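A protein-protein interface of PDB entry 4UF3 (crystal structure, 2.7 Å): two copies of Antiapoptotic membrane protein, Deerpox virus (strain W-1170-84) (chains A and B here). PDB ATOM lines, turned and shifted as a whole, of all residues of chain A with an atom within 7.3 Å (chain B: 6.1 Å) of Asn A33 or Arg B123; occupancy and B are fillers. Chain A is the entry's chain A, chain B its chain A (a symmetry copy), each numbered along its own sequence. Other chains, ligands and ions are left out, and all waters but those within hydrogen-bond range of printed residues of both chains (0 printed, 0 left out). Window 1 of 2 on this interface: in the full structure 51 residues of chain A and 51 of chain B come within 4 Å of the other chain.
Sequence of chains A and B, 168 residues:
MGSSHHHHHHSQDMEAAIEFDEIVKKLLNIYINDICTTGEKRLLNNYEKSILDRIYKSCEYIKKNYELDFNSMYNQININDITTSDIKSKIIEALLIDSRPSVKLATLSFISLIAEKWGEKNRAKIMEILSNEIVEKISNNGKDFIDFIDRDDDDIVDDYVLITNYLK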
ATOM      1  N   LEU A  27     -16.484 -19.254  -8.007  1.00  0.00           N
ATOM      2  CA  LEU A  27     -16.793 -18.440  -6.838  1.00  0.00           C
ATOM      3  C   LEU A  27     -17.659 -19.190  -5.829  1.00  0.00           C
ATOM      4  O   LEU A  27     -17.561 -18.951  -4.625  1.00  0.00           O
ATOM      5  CB  LEU A  27     -17.482 -17.140  -7.265  1.00  0.00           C
ATOM      6  CG  LEU A  27     -16.615 -16.187  -8.085  1.00  0.00           C
ATOM      7  CD1 LEU A  27     -17.319 -14.865  -8.287  1.00  0.00           C
ATOM      8  CD2 LEU A  27     -15.262 -15.980  -7.421  1.00  0.00           C
ATOM      9  N   LEU A  28     -18.513 -20.083  -6.323  1.00  0.00           N
ATOM     10  CA  LEU A  28     -19.360 -20.885  -5.449  1.00  0.00           C
ATOM     11  C   LEU A  28     -18.532 -21.863  -4.626  1.00  0.00           C
ATOM     12  O   LEU A  28     -18.682 -21.944  -3.405  1.00  0.00           O
ATOM     13  CB  LEU A  28     -20.413 -21.648  -6.252  1.00  0.00           C
ATOM     14  CG  LEU A  28     -21.610 -20.851  -6.774  1.00  0.00           C
ATOM     15  CD1 LEU A  28     -22.776 -21.778  -7.078  1.00  0.00           C
ATOM     16  CD2 LEU A  28     -22.010 -19.765  -5.795  1.00  0.00           C
ATOM     17  N   ASN A  29     -17.653 -22.598  -5.302  1.00  0.00           N
ATOM     18  CA  ASN A  29     -16.765 -23.553  -4.645  1.00  0.00           C
ATOM     19  C   ASN A  29     -15.893 -22.901  -3.590  1.00  0.00           C
ATOM     20  O   ASN A  29     -15.691 -23.453  -2.510  1.00  0.00           O
ATOM     21  CB  ASN A  29     -15.877 -24.252  -5.674  1.00  0.00           C
ATOM     22  CG  ASN A  29     -16.601 -25.359  -6.413  1.00  0.00           C
ATOM     23  OD1 ASN A  29     -17.402 -26.092  -5.831  1.00  0.00           O
ATOM     24  ND2 ASN A  29     -16.325 -25.484  -7.708  1.00  0.00           N
ATOM     25  N   ILE A  30     -15.370 -21.724  -3.916  1.00  0.00           N
ATOM     26  CA  ILE A  30     -14.633 -20.932  -2.942  1.00  0.00           C
ATOM     27  C   ILE A  30     -15.543 -20.537  -1.780  1.00  0.00           C
ATOM     28  O   ILE A  30     -15.176 -20.678  -0.608  1.00  0.00           O
ATOM     29  CB  ILE A  30     -14.037 -19.656  -3.564  1.00  0.00           C
ATOM     30  CG1 ILE A  30     -12.886 -20.000  -4.517  1.00  0.00           C
ATOM     31  CG2 ILE A  30     -13.564 -18.711  -2.466  1.00  0.00           C
ATOM     32  CD1 ILE A  30     -12.194 -18.771  -5.112  1.00  0.00           C
ATOM     33  N   TYR A  31     -16.734 -20.051  -2.114  1.00  0.00           N
ATOM     34  CA  TYR A  31     -17.663 -19.560  -1.102  1.00  0.00           C
ATOM     35  C   TYR A  31     -18.015 -20.621  -0.061  1.00  0.00           C
ATOM     36  O   TYR A  31     -17.816 -20.417   1.137  1.00  0.00           O
ATOM     37  CB  TYR A  31     -18.946 -19.038  -1.748  1.00  0.00           C
ATOM     38  CG  TYR A  31     -20.014 -18.729  -0.732  1.00  0.00           C
ATOM     39  CD1 TYR A  31     -19.853 -17.687   0.166  1.00  0.00           C
ATOM     40  CD2 TYR A  31     -21.174 -19.490  -0.657  1.00  0.00           C
ATOM     41  CE1 TYR A  31     -20.816 -17.404   1.104  1.00  0.00           C
ATOM     42  CE2 TYR A  31     -22.145 -19.212   0.280  1.00  0.00           C
ATOM     43  CZ  TYR A  31     -21.959 -18.166   1.161  1.00  0.00           C
ATOM     44  OH  TYR A  31     -22.915 -17.872   2.106  1.00  0.00           O
ATOM     45  N   ILE A  32     -18.528 -21.755  -0.526  1.00  0.00           N
ATOM     46  CA  ILE A  32     -18.994 -22.816   0.359  1.00  0.00           C
ATOM     47  C   ILE A  32     -17.847 -23.456   1.143  1.00  0.00           C
ATOM     48  O   ILE A  32     -18.017 -23.824   2.304  1.00  0.00           O
ATOM     49  CB  ILE A  32     -19.770 -23.889  -0.442  1.00  0.00           C
ATOM     50  CG1 ILE A  32     -21.123 -23.329  -0.890  1.00  0.00           C
ATOM     51  CG2 ILE A  32     -19.982 -25.150   0.378  1.00  0.00           C
ATOM     52  CD1 ILE A  32     -22.016 -22.896   0.255  1.00  0.00           C
ATOM     53  N   ASN A  33     -16.679 -23.570   0.517  1.00  0.00           N
ATOM     54  CA  ASN A  33     -15.497 -24.055   1.219  1.00  0.00           C
ATOM     55  C   ASN A  33     -15.130 -23.146   2.387  1.00  0.00           C
ATOM     56  O   ASN A  33     -14.682 -23.611   3.432  1.00  0.00           O
ATOM     57  CB  ASN A  33     -14.307 -24.183   0.265  1.00  0.00           C
ATOM     58  CG  ASN A  33     -14.169 -25.584  -0.311  1.00  0.00           C
ATOM     59  OD1 ASN A  33     -13.897 -26.546   0.411  1.00  0.00           O
ATOM     60  ND2 ASN A  33     -14.342 -25.700  -1.619  1.00  0.00           N
ATOM     61  N   ASP A  34     -15.318 -21.844   2.204  1.00  0.00           N
ATOM     62  CA  ASP A  34     -15.020 -20.881   3.257  1.00  0.00           C
ATOM     63  C   ASP A  34     -16.062 -20.977   4.365  1.00  0.00           C
ATOM     64  O   ASP A  34     -15.774 -20.702   5.531  1.00  0.00           O
ATOM     65  CB  ASP A  34     -14.968 -19.463   2.689  1.00  0.00           C
ATOM     66  CG  ASP A  34     -14.338 -18.472   3.644  1.00  0.00           C
ATOM     67  OD1 ASP A  34     -13.103 -18.297   3.590  1.00  0.00           O
ATOM     68  OD2 ASP A  34     -15.077 -17.864   4.446  1.00  0.00           O
ATOM     69  N   ILE A  35     -17.272 -21.387   3.990  1.00  0.00           N
ATOM     70  CA  ILE A  35     -18.382 -21.514   4.931  1.00  0.00           C
ATOM     71  C   ILE A  35     -18.244 -22.775   5.783  1.00  0.00           C
ATOM     72  O   ILE A  35     -18.592 -22.779   6.963  1.00  0.00           O
ATOM     73  CB  ILE A  35     -19.739 -21.536   4.196  1.00  0.00           C
ATOM     74  CG1 ILE A  35     -19.979 -20.200   3.493  1.00  0.00           C
ATOM     75  CG2 ILE A  35     -20.882 -21.822   5.159  1.00  0.00           C
ATOM     76  CD1 ILE A  35     -19.992 -19.015   4.441  1.00  0.00           C
ATOM     77  N   CYS A  36     -17.733 -23.847   5.183  1.00  0.00           N
ATOM     78  CA  CYS A  36     -17.452 -25.074   5.926  1.00  0.00           C
ATOM     79  C   CYS A  36     -16.405 -24.795   6.995  1.00  0.00           C
ATOM     80  O   CYS A  36     -16.580 -25.147   8.163  1.00  0.00           O
ATOM     81  CB  CYS A  36     -16.962 -26.185   4.999  1.00  0.00           C
ATOM     82  SG  CYS A  36     -18.125 -26.686   3.721  1.00  0.00           S
ATOM     83  N   THR A  37     -15.321 -24.149   6.573  1.00  0.00           N
ATOM     84  CA  THR A  37     -14.239 -23.750   7.465  1.00  0.00           C
ATOM     85  C   THR A  37     -14.749 -22.930   8.650  1.00  0.00           C
ATOM     86  O   THR A  37     -14.307 -23.118   9.783  1.00  0.00           O
ATOM     87  CB  THR A  37     -13.169 -22.936   6.701  1.00  0.00           C
ATOM     88  OG1 THR A  37     -12.565 -23.761   5.695  1.00  0.00           O
ATOM     89  CG2 THR A  37     -12.096 -22.427   7.645  1.00  0.00           C
ATOM     90  N   THR A  38     -15.685 -22.026   8.386  1.00  0.00           N
ATOM     91  CA  THR A  38     -16.267 -21.204   9.439  1.00  0.00           C
ATOM     92  C   THR A  38     -17.131 -22.047  10.372  1.00  0.00           C
ATOM     93  O   THR A  38     -17.130 -21.845  11.588  1.00  0.00           O
ATOM     94  CB  THR A  38     -17.109 -20.057   8.847  1.00  0.00           C
ATOM     95  OG1 THR A  38     -16.281 -19.248   8.003  1.00  0.00           O
ATOM     96  CG2 THR A  38     -17.697 -19.190   9.954  1.00  0.00           C
ATOM     97  N   GLY A  39     -17.856 -22.999   9.796  1.00  0.00           N
ATOM     98  CA  GLY A  39     -18.676 -23.903  10.577  1.00  0.00           C
ATOM     99  C   GLY A  39     -17.823 -24.765  11.486  1.00  0.00           C
ATOM    100  O   GLY A  39     -18.206 -25.056  12.618  1.00  0.00           O
ATOM    101  N   GLU A  40     -16.656 -25.164  10.991  1.00  0.00           N
ATOM    102  CA  GLU A  40     -15.752 -26.009  11.757  1.00  0.00           C
ATOM    103  C   GLU A  40     -15.063 -25.230  12.875  1.00  0.00           C
ATOM    104  O   GLU A  40     -14.913 -25.740  13.984  1.00  0.00           O
ATOM    105  CB  GLU A  40     -14.715 -26.651  10.832  1.00  0.00           C
ATOM    106  CG  GLU A  40     -15.311 -27.635   9.831  1.00  0.00           C
ATOM    107  CD  GLU A  40     -14.412 -27.878   8.632  1.00  0.00           C
ATOM    108  OE1 GLU A  40     -13.306 -27.296   8.587  1.00  0.00           O
ATOM    109  OE2 GLU A  40     -14.819 -28.641   7.730  1.00  0.00           O
ATOM    110  N   ARG A 123      -7.987 -27.542  -4.868  1.00  0.00           N
ATOM    111  CA  ARG A 123      -7.775 -27.658  -3.431  1.00  0.00           C
ATOM    112  C   ARG A 123      -7.378 -29.083  -3.057  1.00  0.00           C
ATOM    113  O   ARG A 123      -6.581 -29.298  -2.143  1.00  0.00           O
ATOM    114  CB  ARG A 123      -9.042 -27.235  -2.681  1.00  0.00           C
ATOM    115  CG  ARG A 123      -9.154 -27.753  -1.255  1.00  0.00           C
ATOM    116  CD  ARG A 123     -10.529 -27.436  -0.678  1.00  0.00           C
ATOM    117  NE  ARG A 123     -10.870 -26.032  -0.860  1.00  0.00           N
ATOM    118  CZ  ARG A 123     -10.608 -25.078   0.027  1.00  0.00           C
ATOM    119  NH1 ARG A 123     -10.008 -25.378   1.171  1.00  0.00           N
ATOM    120  NH2 ARG A 123     -10.950 -23.821  -0.227  1.00  0.00           N
ATOM    121  N   MET A 127      -4.387 -30.812  -0.754  1.00  0.00           N
ATOM    122  CA  MET A 127      -4.728 -31.670   0.374  1.00  0.00           C
ATOM    123  C   MET A 127      -4.126 -33.065   0.241  1.00  0.00           C
ATOM    124  O   MET A 127      -3.929 -33.754   1.241  1.00  0.00           O
ATOM    125  CB  MET A 127      -6.248 -31.778   0.532  1.00  0.00           C
ATOM    126  CG  MET A 127      -6.944 -30.457   0.827  1.00  0.00           C
ATOM    127  SD  MET A 127      -6.127 -29.507   2.121  1.00  0.00           S
ATOM    128  CE  MET A 127      -6.307 -30.605   3.521  1.00  0.00           C
ATOM    129  N   ASN B  29      -5.913 -29.734   9.474  1.00  0.00           N
ATOM    130  CA  ASN B  29      -6.829 -29.814   8.341  1.00  0.00           C
ATOM    131  C   ASN B  29      -7.649 -28.550   8.169  1.00  0.00           C
ATOM    132  O   ASN B  29      -7.853 -28.078   7.053  1.00  0.00           O
ATOM    133  CB  ASN B  29      -7.768 -31.010   8.496  1.00  0.00           C
ATOM    134  CG  ASN B  29      -7.110 -32.322   8.119  1.00  0.00           C
ATOM    135  OD1 ASN B  29      -6.330 -32.389   7.167  1.00  0.00           O
ATOM    136  ND2 ASN B  29      -7.417 -33.374   8.870  1.00  0.00           N
ATOM    137  N   ILE B  30      -8.125 -28.011   9.286  1.00  0.00           N
ATOM    138  CA  ILE B  30      -8.805 -26.725   9.272  1.00  0.00           C
ATOM    139  C   ILE B  30      -7.854 -25.627   8.799  1.00  0.00           C
ATOM    140  O   ILE B  30      -8.204 -24.811   7.939  1.00  0.00           O
ATOM    141  CB  ILE B  30      -9.357 -26.344  10.657  1.00  0.00           C
ATOM    142  CG1 ILE B  30     -10.541 -27.240  11.040  1.00  0.00           C
ATOM    143  CG2 ILE B  30      -9.764 -24.876  10.673  1.00  0.00           C
ATOM    144  CD1 ILE B  30     -11.189 -26.866  12.374  1.00  0.00           C
ATOM    145  N   ASN B  33      -6.808 -25.896   4.978  1.00  0.00           N
ATOM    146  CA  ASN B  33      -7.996 -25.624   4.178  1.00  0.00           C
ATOM    147  C   ASN B  33      -8.298 -24.130   4.119  1.00  0.00           C
ATOM    148  O   ASN B  33      -8.745 -23.617   3.095  1.00  0.00           O
ATOM    149  CB  ASN B  33      -9.210 -26.379   4.725  1.00  0.00           C
ATOM    150  CG  ASN B  33      -9.423 -27.718   4.036  1.00  0.00           C
ATOM    151  OD1 ASN B  33      -9.723 -27.781   2.842  1.00  0.00           O
ATOM    152  ND2 ASN B  33      -9.282 -28.797   4.794  1.00  0.00           N
ATOM    153  N   ASP B  34      -8.055 -23.434   5.224  1.00  0.00           N
ATOM    154  CA  ASP B  34      -8.289 -21.996   5.278  1.00  0.00           C
ATOM    155  C   ASP B  34      -7.229 -21.263   4.464  1.00  0.00           C
ATOM    156  O   ASP B  34      -7.480 -20.185   3.923  1.00  0.00           O
ATOM    157  CB  ASP B  34      -8.288 -21.507   6.726  1.00  0.00           C
ATOM    158  CG  ASP B  34      -8.853 -20.111   6.873  1.00  0.00           C
ATOM    159  OD1 ASP B  34     -10.081 -19.983   7.067  1.00  0.00           O
ATOM    160  OD2 ASP B  34      -8.072 -19.140   6.799  1.00  0.00           O
ATOM    161  N   THR B  37      -8.065 -21.606   0.634  1.00  0.00           N
ATOM    162  CA  THR B  37      -9.110 -20.621   0.382  1.00  0.00           C
ATOM    163  C   THR B  37      -8.540 -19.212   0.224  1.00  0.00           C
ATOM    164  O   THR B  37      -8.965 -18.453  -0.645  1.00  0.00           O
ATOM    165  CB  THR B  37     -10.158 -20.627   1.518  1.00  0.00           C
ATOM    166  OG1 THR B  37     -10.819 -21.900   1.556  1.00  0.00           O
ATOM    167  CG2 THR B  37     -11.188 -19.531   1.314  1.00  0.00           C
ATOM    168  N   GLU B  40      -6.686 -18.964  -3.033  1.00  0.00           N
ATOM    169  CA  GLU B  40      -7.611 -18.889  -4.155  1.00  0.00           C
ATOM    170  C   GLU B  40      -8.242 -17.503  -4.275  1.00  0.00           C
ATOM    171  O   GLU B  40      -8.391 -16.985  -5.379  1.00  0.00           O
ATOM    172  CB  GLU B  40      -8.695 -19.962  -4.021  1.00  0.00           C
ATOM    173  CG  GLU B  40      -8.165 -21.388  -4.131  1.00  0.00           C
ATOM    174  CD  GLU B  40      -9.098 -22.416  -3.520  1.00  0.00           C
ATOM    175  OE1 GLU B  40     -10.177 -22.024  -3.024  1.00  0.00           O
ATOM    176  OE2 GLU B  40      -8.744 -23.615  -3.522  1.00  0.00           O
ATOM    177  N   TRP B 118     -22.548 -28.253   9.975  1.00  0.00           N
ATOM    178  CA  TRP B 118     -21.829 -29.518   9.872  1.00  0.00           C
ATOM    179  C   TRP B 118     -20.323 -29.315  10.026  1.00  0.00           C
ATOM    180  O   TRP B 118     -19.529 -29.823   9.232  1.00  0.00           O
ATOM    181  CB  TRP B 118     -22.154 -30.206   8.544  1.00  0.00           C
ATOM    182  CG  TRP B 118     -23.538 -30.802   8.518  1.00  0.00           C
ATOM    183  CD1 TRP B 118     -24.463 -30.766   9.521  1.00  0.00           C
ATOM    184  CD2 TRP B 118     -24.145 -31.533   7.440  1.00  0.00           C
ATOM    185  NE1 TRP B 118     -25.605 -31.423   9.134  1.00  0.00           N
ATOM    186  CE2 TRP B 118     -25.437 -31.901   7.864  1.00  0.00           C
ATOM    187  CE3 TRP B 118     -23.720 -31.907   6.163  1.00  0.00           C
ATOM    188  CZ2 TRP B 118     -26.309 -32.625   7.052  1.00  0.00           C
ATOM    189  CZ3 TRP B 118     -24.588 -32.627   5.359  1.00  0.00           C
ATOM    190  CH2 TRP B 118     -25.868 -32.978   5.807  1.00  0.00           C
ATOM    191  N   LYS B 121     -18.687 -32.703  11.030  1.00  0.00           N
ATOM    192  CA  LYS B 121     -18.714 -33.694   9.962  1.00  0.00           C
ATOM    193  C   LYS B 121     -17.605 -33.379   8.970  1.00  0.00           C
ATOM    194  O   LYS B 121     -16.962 -32.333   9.061  1.00  0.00           O
ATOM    195  CB  LYS B 121     -20.071 -33.713   9.255  1.00  0.00           C
ATOM    196  CG  LYS B 121     -21.225 -34.192  10.115  1.00  0.00           C
ATOM    197  CD  LYS B 121     -22.556 -33.941   9.425  1.00  0.00           C
ATOM    198  CE  LYS B 121     -22.717 -34.794   8.176  1.00  0.00           C
ATOM    199  NZ  LYS B 121     -22.912 -36.233   8.519  1.00  0.00           N
ATOM    200  N   ASN B 122     -17.387 -34.277   8.017  1.00  0.00           N
ATOM    201  CA  ASN B 122     -16.346 -34.072   7.021  1.00  0.00           C
ATOM    202  C   ASN B 122     -16.746 -33.008   6.007  1.00  0.00           C
ATOM    203  O   ASN B 122     -17.899 -32.941   5.583  1.00  0.00           O
ATOM    204  CB  ASN B 122     -16.017 -35.383   6.304  1.00  0.00           C
ATOM    205  CG  ASN B 122     -14.698 -35.324   5.546  1.00  0.00           C
ATOM    206  OD1 ASN B 122     -14.276 -34.263   5.083  1.00  0.00           O
ATOM    207  ND2 ASN B 122     -14.038 -36.470   5.420  1.00  0.00           N
ATOM    208  N   ARG B 123     -15.779 -32.176   5.634  1.00  0.00           N
ATOM    209  CA  ARG B 123     -15.966 -31.148   4.617  1.00  0.00           C
ATOM    210  C   ARG B 123     -16.419 -31.770   3.299  1.00  0.00           C
ATOM    211  O   ARG B 123     -17.206 -31.179   2.559  1.00  0.00           O
ATOM    212  CB  ARG B 123     -14.666 -30.361   4.426  1.00  0.00           C
ATOM    213  CG  ARG B 123     -14.548 -29.617   3.104  1.00  0.00           C
ATOM    214  CD  ARG B 123     -13.149 -29.035   2.941  1.00  0.00           C
ATOM    215  NE  ARG B 123     -12.749 -28.279   4.120  1.00  0.00           N
ATOM    216  CZ  ARG B 123     -12.949 -26.975   4.275  1.00  0.00           C
ATOM    217  NH1 ARG B 123     -13.538 -26.272   3.317  1.00  0.00           N
ATOM    218  NH2 ARG B 123     -12.557 -26.369   5.389  1.00  0.00           N
ATOM    219  N   ALA B 124     -15.917 -32.970   3.020  1.00  0.00           N
ATOM    220  CA  ALA B 124     -16.296 -33.713   1.825  1.00  0.00           C
ATOM    221  C   ALA B 124     -17.790 -34.028   1.815  1.00  0.00           C
ATOM    222  O   ALA B 124     -18.431 -33.992   0.764  1.00  0.00           O
ATOM    223  CB  ALA B 124     -15.485 -34.995   1.723  1.00  0.00           C
ATOM    224  N   LYS B 125     -18.338 -34.331   2.988  1.00  0.00           N
ATOM    225  CA  LYS B 125     -19.762 -34.628   3.120  1.00  0.00           C
ATOM    226  C   LYS B 125     -20.627 -33.449   2.691  1.00  0.00           C
ATOM    227  O   LYS B 125     -21.725 -33.629   2.167  1.00  0.00           O
ATOM    228  CB  LYS B 125     -20.105 -35.017   4.558  1.00  0.00           C
ATOM    229  CG  LYS B 125     -19.803 -36.460   4.901  1.00  0.00           C
ATOM    230  CD  LYS B 125     -20.368 -36.815   6.262  1.00  0.00           C
ATOM    231  CE  LYS B 125     -20.191 -38.290   6.573  1.00  0.00           C
ATOM    232  NZ  LYS B 125     -20.798 -38.649   7.884  1.00  0.00           N
ATOM    233  N   ILE B 126     -20.126 -32.242   2.923  1.00  0.00           N
ATOM    234  CA  ILE B 126     -20.840 -31.039   2.530  1.00  0.00           C
ATOM    235  C   ILE B 126     -20.647 -30.761   1.041  1.00  0.00           C
ATOM    236  O   ILE B 126     -21.578 -30.345   0.350  1.00  0.00           O
ATOM    237  CB  ILE B 126     -20.373 -29.818   3.347  1.00  0.00           C
ATOM    238  CG1 ILE B 126     -20.497 -30.097   4.847  1.00  0.00           C
ATOM    239  CG2 ILE B 126     -21.163 -28.585   2.953  1.00  0.00           C
ATOM    240  CD1 ILE B 126     -19.936 -28.995   5.724  1.00  0.00           C
ATOM    241  N   MET B 127     -19.436 -31.005   0.551  1.00  0.00           N
ATOM    242  CA  MET B 127     -19.110 -30.719  -0.841  1.00  0.00           C
ATOM    243  C   MET B 127     -19.776 -31.698  -1.803  1.00  0.00           C
ATOM    244  O   MET B 127     -19.984 -31.375  -2.972  1.00  0.00           O
ATOM    245  CB  MET B 127     -17.594 -30.737  -1.057  1.00  0.00           C
ATOM    246  CG  MET B 127     -16.833 -29.688  -0.259  1.00  0.00           C
ATOM    247  SD  MET B 127     -17.580 -28.052  -0.359  1.00  0.00           S
ATOM    248  CE  MET B 127     -17.421 -27.707  -2.107  1.00  0.00           C
ATOM    249  N   GLU B 128     -20.107 -32.892  -1.321  1.00  0.00           N
ATOM    250  CA  GLU B 128     -20.750 -33.879  -2.181  1.00  0.00           C
ATOM    251  C   GLU B 128     -22.237 -33.575  -2.330  1.00  0.00           C
ATOM    252  O   GLU B 128     -22.930 -34.203  -3.129  1.00  0.00           O
ATOM    253  CB  GLU B 128     -20.540 -35.297  -1.647  1.00  0.00           C
ATOM    254  CG  GLU B 128     -21.163 -35.579  -0.295  1.00  0.00           C
ATOM    255  CD  GLU B 128     -20.989 -37.029   0.120  1.00  0.00           C
ATOM    256  OE1 GLU B 128     -20.881 -37.897  -0.773  1.00  0.00           O
ATOM    257  OE2 GLU B 128     -20.956 -37.301   1.340  1.00  0.00           O
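Asn A33 touches just these residues of chain B: Arg B123 (2.9 Å) and Met B127 (3.7 Å). Arg B123 touches just these residues of chain A: Asn A33, Cys A36, Thr A37 and Glu A40. Of the printed residues of chain A, Glu B40 touches Ile A30 (3.7 Å) and Arg A123 (3.4 Å). Of the printed residues of chain A, Asn B33 touches Arg A123 and Met A127. Of the printed residues of chain B, Thr A37 touches Asp B34 (3.2 Å) and Arg B123 (2.6 Å). Of the printed residues of chain A, Ile B126 touches Cys A36 (3.6 Å). Glu B128 touches none of the printed residues of chain A. Lys B121 touches none of the printed residues of chain A. The nearest residue of chain B that does not touch Asn A33 is Thr B37 (4.4 Å). The nearest residue of chain A that does not touch Arg B123 is Arg A123 (4.2 Å).
The side-chain amide oxygen (OD1) of Asn A33 sits at hydrogen-bond distance from the guanidinium group (NE) of Arg A123 (3.3 Å). The backbone carbonyl oxygen of Asn A33 lies within hydrogen-bond range of the side-chain hydroxyl of Thr A37 (3.1 Å). OD1 of Asn B33 lies within hydrogen-bond range of NE of Arg B123 (3.3 Å). OG1 of Thr B37 sits at hydrogen-bond distance from O of Asn B33 (3.1 Å). O of Asn A29 lies within hydrogen-bond range of ND2 of Asn A33 (2.8 Å). The backbone carbonyl oxygen (O) of Ile A32 sits at hydrogen-bond distance from the side-chain sulfur (SG) of Cys A36 (3.2 Å).
Of the 15 printed residues of chain B, 8 touch a printed residue of chain A. Printed residues of chain B that touch a printed residue of chain A: Ile B30, Asn B33, Asp B34, Thr B37, Glu B40, Arg B123, Ile B126 and Met B127. Hydrophobic or aromatic side chains of chain B within 4 Å of the printed part of chain A: Ile B30, Ile B126 and Met B127. Printed residues of chain A that touch a printed residue of chain B: Ile A30, Ile A32, Asn A33, Asp A34, Cys A36, Thr A37, Glu A40, Arg A123 and Met A127. Hydrophobic or aromatic side chains of chain A that line the printed part of chain B: Ile A30, Ile A32 and Met A127.
The side-chain hydroxyl (OG1) of Thr A37 sits at hydrogen-bond distance from the guanidinium group (NH2) of Arg B123. The side-chain carboxylate (OE1) of Glu B40 lies within salt-bridge range of the guanidinium group (NH2) of Arg A123 (3.4 Å). The guanidinium group (NH1) of Arg A123 sits at hydrogen-bond distance from the backbone carbonyl oxygen (O) of Asn B33 (2.9 Å). NH2 of Arg B123 is in salt-bridge range of OE1 of Glu A40. OG1 of Thr B37 lies within hydrogen-bond range of NH2 of Arg A123. The guanidinium group (NH1) of Arg B123 is in hydrogen-bond range of the backbone carbonyl oxygen (O) of Asn A33, 2.9 Å away.
Ile A30 touches Glu B40 (CG1 to OE1, 3.7 Å). Met B127 touches Ile A32. ND2 of Asn A33 touches CE of Met B127, 3.7 Å away. OD1 of Asp A34 touches CG2 of Thr B37, 3.2 Å away. Arg B123 touches Cys A36 (NH1 to CB, 3.8 Å). Ile B126 touches Cys A36. CG2 of Thr A37 touches OD1 of Asp B34 (3.2 Å). Ile B30 touches Glu A40. Asn B33 touches Met A127 (ND2 to CE, 3.7 Å).
Asn A33 touches Arg B123, and with the chains exchanged Arg A123 touches Asn B33. Asp A34 touches Thr B37, and with the chains exchanged Thr A37 touches Asp B34. Thr A37 touches Arg B123, and with the chains exchanged Arg A123 touches Thr B37. Glu A40 touches Arg B123, and with the chains exchanged Arg A123 touches Glu B40. Of the 15 pairs that touch across the chains among the printed residues, 12 have their exchanged pair printed and touching as well.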
